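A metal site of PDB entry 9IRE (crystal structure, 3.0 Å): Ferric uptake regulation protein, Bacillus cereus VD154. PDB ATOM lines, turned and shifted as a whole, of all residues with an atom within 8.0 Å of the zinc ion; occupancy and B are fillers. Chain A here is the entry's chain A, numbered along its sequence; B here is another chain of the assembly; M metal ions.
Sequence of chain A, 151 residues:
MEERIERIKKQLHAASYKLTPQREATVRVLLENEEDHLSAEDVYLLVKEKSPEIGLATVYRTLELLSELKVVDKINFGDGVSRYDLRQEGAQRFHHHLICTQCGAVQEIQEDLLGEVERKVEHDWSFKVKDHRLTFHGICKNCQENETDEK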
ATOM      1  N   ILE A  99       8.338  17.289  25.257  1.00  0.00           N
ATOM      2  CA  ILE A  99       9.570  17.450  24.504  1.00  0.00           C
ATOM      3  C   ILE A  99       9.914  18.932  24.470  1.00  0.00           C
ATOM      4  O   ILE A  99       9.022  19.793  24.390  1.00  0.00           O
ATOM      5  CB  ILE A  99       9.397  16.902  23.088  1.00  0.00           C
ATOM      6  CG1 ILE A  99       8.926  15.453  23.141  1.00  0.00           C
ATOM      7  CG2 ILE A  99      10.672  17.058  22.321  1.00  0.00           C
ATOM      8  CD1 ILE A  99       8.414  14.949  21.829  1.00  0.00           C
ATOM      9  N   CYS A 100      11.199  19.235  24.563  1.00  0.00           N
ATOM     10  CA  CYS A 100      11.715  20.590  24.420  1.00  0.00           C
ATOM     11  C   CYS A 100      12.237  20.776  23.004  1.00  0.00           C
ATOM     12  O   CYS A 100      12.951  19.916  22.474  1.00  0.00           O
ATOM     13  CB  CYS A 100      12.828  20.830  25.436  1.00  0.00           C
ATOM     14  SG  CYS A 100      13.256  22.531  25.536  1.00  0.00           S
ATOM     15  N   THR A 101      11.846  21.874  22.371  1.00  0.00           N
ATOM     16  CA  THR A 101      12.239  22.110  20.988  1.00  0.00           C
ATOM     17  C   THR A 101      13.439  23.033  20.922  1.00  0.00           C
ATOM     18  O   THR A 101      13.372  24.135  20.375  1.00  0.00           O
ATOM     19  CB  THR A 101      11.083  22.723  20.202  1.00  0.00           C
ATOM     20  OG1 THR A 101      10.695  23.949  20.827  1.00  0.00           O
ATOM     21  CG2 THR A 101       9.888  21.781  20.170  1.00  0.00           C
ATOM     22  N   GLN A 102      14.551  22.561  21.457  1.00  0.00           N
ATOM     23  CA  GLN A 102      15.743  23.386  21.578  1.00  0.00           C
ATOM     24  C   GLN A 102      16.796  22.539  22.266  1.00  0.00           C
ATOM     25  O   GLN A 102      17.569  21.832  21.615  1.00  0.00           O
ATOM     26  CB  GLN A 102      15.427  24.646  22.376  1.00  0.00           C
ATOM     27  CG  GLN A 102      16.616  25.513  22.683  1.00  0.00           C
ATOM     28  CD  GLN A 102      16.466  26.185  24.021  1.00  0.00           C
ATOM     29  OE1 GLN A 102      15.561  26.997  24.231  1.00  0.00           O
ATOM     30  NE2 GLN A 102      17.341  25.824  24.967  1.00  0.00           N
ATOM     31  N   CYS A 103      16.764  22.573  23.604  1.00  0.00           N
ATOM     32  CA  CYS A 103      17.627  21.696  24.405  1.00  0.00           C
ATOM     33  C   CYS A 103      17.319  20.228  24.104  1.00  0.00           C
ATOM     34  O   CYS A 103      18.240  19.399  24.034  1.00  0.00           O
ATOM     35  CB  CYS A 103      17.442  22.013  25.891  1.00  0.00           C
ATOM     36  SG  CYS A 103      16.070  21.162  26.712  1.00  0.00           S
ATOM     37  N   GLY A 104      16.039  19.899  23.901  1.00  0.00           N
ATOM     38  CA  GLY A 104      15.632  18.551  23.552  1.00  0.00           C
ATOM     39  C   GLY A 104      15.398  17.610  24.724  1.00  0.00           C
ATOM     40  O   GLY A 104      15.539  16.398  24.550  1.00  0.00           O
ATOM     41  N   ALA A 105      15.075  18.139  25.902  1.00  0.00           N
ATOM     42  CA  ALA A 105      14.697  17.294  27.024  1.00  0.00           C
ATOM     43  C   ALA A 105      13.349  16.626  26.761  1.00  0.00           C
ATOM     44  O   ALA A 105      12.481  17.158  26.058  1.00  0.00           O
ATOM     45  CB  ALA A 105      14.654  18.109  28.300  1.00  0.00           C
ATOM     46  N   VAL A 106      13.172  15.442  27.345  1.00  0.00           N
ATOM     47  CA  VAL A 106      11.942  14.684  27.213  1.00  0.00           C
ATOM     48  C   VAL A 106      11.520  14.265  28.609  1.00  0.00           C
ATOM     49  O   VAL A 106      12.304  13.649  29.335  1.00  0.00           O
ATOM     50  CB  VAL A 106      12.148  13.438  26.344  1.00  0.00           C
ATOM     51  CG1 VAL A 106      10.879  12.676  26.222  1.00  0.00           C
ATOM     52  CG2 VAL A 106      12.712  13.785  24.980  1.00  0.00           C
ATOM     53  N   GLN A 107      10.274  14.585  28.974  1.00  0.00           N
ATOM     54  CA  GLN A 107       9.735  14.257  30.290  1.00  0.00           C
ATOM     55  C   GLN A 107       8.573  13.290  30.130  1.00  0.00           C
ATOM     56  O   GLN A 107       7.481  13.681  29.693  1.00  0.00           O
ATOM     57  CB  GLN A 107       9.267  15.507  31.026  1.00  0.00           C
ATOM     58  CG  GLN A 107      10.195  16.015  32.124  1.00  0.00           C
ATOM     59  CD  GLN A 107      10.062  17.516  32.263  1.00  0.00           C
ATOM     60  OE1 GLN A 107       8.969  18.051  32.130  1.00  0.00           O
ATOM     61  NE2 GLN A 107      11.177  18.205  32.450  1.00  0.00           N
ATOM     62  N   GLY A 138       7.383  22.494  23.340  1.00  0.00           N
ATOM     63  CA  GLY A 138       7.520  23.796  23.950  1.00  0.00           C
ATOM     64  C   GLY A 138       8.844  23.993  24.647  1.00  0.00           C
ATOM     65  O   GLY A 138       9.428  23.042  25.171  1.00  0.00           O
ATOM     66  N   ILE A 139       9.374  25.206  24.626  1.00  0.00           N
ATOM     67  CA  ILE A 139      10.662  25.429  25.253  1.00  0.00           C
ATOM     68  C   ILE A 139      10.485  25.252  26.760  1.00  0.00           C
ATOM     69  O   ILE A 139       9.534  25.787  27.365  1.00  0.00           O
ATOM     70  CB  ILE A 139      11.237  26.786  24.810  1.00  0.00           C
ATOM     71  CG1 ILE A 139      11.912  26.626  23.425  1.00  0.00           C
ATOM     72  CG2 ILE A 139      12.162  27.382  25.847  1.00  0.00           C
ATOM     73  CD1 ILE A 139      12.448  27.906  22.708  1.00  0.00           C
ATOM     74  N   CYS A 140      11.342  24.409  27.358  1.00  0.00           N
ATOM     75  CA  CYS A 140      11.090  23.873  28.699  1.00  0.00           C
ATOM     76  C   CYS A 140      11.480  24.842  29.829  1.00  0.00           C
ATOM     77  O   CYS A 140      11.979  25.952  29.614  1.00  0.00           O
ATOM     78  CB  CYS A 140      11.842  22.560  28.881  1.00  0.00           C
ATOM     79  SG  CYS A 140      13.607  22.843  29.179  1.00  0.00           S
ATOM     80  N   LYS A 141      11.266  24.374  31.064  1.00  0.00           N
ATOM     81  CA  LYS A 141      11.366  25.236  32.231  1.00  0.00           C
ATOM     82  C   LYS A 141      12.692  25.946  32.286  1.00  0.00           C
ATOM     83  O   LYS A 141      12.749  27.160  32.476  1.00  0.00           O
ATOM     84  CB  LYS A 141      11.187  24.434  33.523  1.00  0.00           C
ATOM     85  CG  LYS A 141      11.498  25.269  34.761  1.00  0.00           C
ATOM     86  CD  LYS A 141      11.185  24.518  36.026  1.00  0.00           C
ATOM     87  CE  LYS A 141      11.444  25.387  37.232  1.00  0.00           C
ATOM     88  NZ  LYS A 141      10.811  24.821  38.479  1.00  0.00           N
ATOM     89  N   ASN A 142      13.773  25.179  32.157  1.00  0.00           N
ATOM     90  CA  ASN A 142      15.118  25.713  32.298  1.00  0.00           C
ATOM     91  C   ASN A 142      15.575  26.510  31.072  1.00  0.00           C
ATOM     92  O   ASN A 142      16.490  27.324  31.198  1.00  0.00           O
ATOM     93  CB  ASN A 142      16.110  24.572  32.561  1.00  0.00           C
ATOM     94  CG  ASN A 142      16.324  24.308  34.027  1.00  0.00           C
ATOM     95  OD1 ASN A 142      16.082  23.196  34.494  1.00  0.00           O
ATOM     96  ND2 ASN A 142      16.779  25.315  34.755  1.00  0.00           N
ATOM     97  N   CYS A 143      14.971  26.290  29.891  1.00  0.00           N
ATOM     98  CA  CYS A 143      15.280  27.138  28.757  1.00  0.00           C
ATOM     99  C   CYS A 143      14.547  28.458  28.802  1.00  0.00           C
ATOM    100  O   CYS A 143      14.822  29.331  27.976  1.00  0.00           O
ATOM    101  CB  CYS A 143      14.965  26.447  27.446  1.00  0.00           C
ATOM    102  SG  CYS A 143      15.894  24.958  27.236  1.00  0.00           S
ATOM    103  N   GLN A 144      13.612  28.637  29.718  1.00  0.00           N
ATOM    104  CA  GLN A 144      13.065  29.959  29.951  1.00  0.00           C
ATOM    105  C   GLN A 144      14.047  30.827  30.717  1.00  0.00           C
ATOM    106  O   GLN A 144      14.093  32.047  30.501  1.00  0.00           O
ATOM    107  CB  GLN A 144      11.717  29.847  30.660  1.00  0.00           C
ATOM    108  CG  GLN A 144      10.672  29.256  29.721  1.00  0.00           C
ATOM    109  CD  GLN A 144       9.515  28.613  30.436  1.00  0.00           C
ATOM    110  OE1 GLN A 144       8.702  29.285  31.093  1.00  0.00           O
ATOM    111  NE2 GLN A 144       9.406  27.298  30.288  1.00  0.00           N
ATOM    112  N   ASN A 146      17.549  30.298  31.015  1.00  0.00           N
ATOM    113  CA  ASN A 146      18.901  30.368  30.488  1.00  0.00           C
ATOM    114  C   ASN A 146      18.976  31.104  29.164  1.00  0.00           C
ATOM    115  O   ASN A 146      20.081  31.322  28.645  1.00  0.00           O
ATOM    116  CB  ASN A 146      19.498  28.958  30.333  1.00  0.00           C
ATOM    117  CG  ASN A 146      19.684  28.289  31.665  1.00  0.00           C
ATOM    118  OD1 ASN A 146      19.727  28.950  32.703  1.00  0.00           O
ATOM    119  ND2 ASN A 146      19.815  26.971  31.657  1.00  0.00           N
ATOM    120  N   PHE B 127       6.353  24.571  32.070  1.00  0.00           N
ATOM    121  CA  PHE B 127       6.624  24.290  30.680  1.00  0.00           C
ATOM    122  C   PHE B 127       5.825  25.277  29.855  1.00  0.00           C
ATOM    123  O   PHE B 127       4.685  25.623  30.203  1.00  0.00           O
ATOM    124  CB  PHE B 127       6.208  22.860  30.352  1.00  0.00           C
ATOM    125  CG  PHE B 127       6.888  22.270  29.167  1.00  0.00           C
ATOM    126  CD1 PHE B 127       8.154  21.751  29.273  1.00  0.00           C
ATOM    127  CD2 PHE B 127       6.233  22.170  27.955  1.00  0.00           C
ATOM    128  CE1 PHE B 127       8.766  21.163  28.171  1.00  0.00           C
ATOM    129  CE2 PHE B 127       6.842  21.577  26.874  1.00  0.00           C
ATOM    130  CZ  PHE B 127       8.099  21.078  26.975  1.00  0.00           C
HETATM  131 ZN    ZN M   1      14.761  22.908  27.216  1.00  0.00          ZN
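The zinc ion is bound by the side-chain sulfur (SG) of Cys 103 (2.2 Å), the side-chain sulfur (SG) of Cys 140 (2.3 Å), the side-chain sulfur (SG) of Cys 100 (2.3 Å) and the side-chain sulfur (SG) of Cys 143 (2.3 Å).
Four residues have an atom within 4 Å of the zinc ion: Cys 100, Cys 103, Cys 140 and Cys 143. The nearest printed residue that does not touch the zinc ion is Gln 102 (4.5 Å).
N of Cys 100 sits at hydrogen-bond distance from O of Ala 105 (2.9 Å). The backbone carbonyl oxygen (O) of Cys 140 is in hydrogen-bond range of the side-chain amide nitrogen (NE2) of Gln 144, 3.0 Å away. SG of Cys 103 lies close to N of Ala 105, 3.3 Å away. The side-chain amide nitrogen of Gln 102 lies close to the side-chain sulfur of Cys 143. The side-chain sulfur of Cys 140 sits close to the backbone NH of Asn 142.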
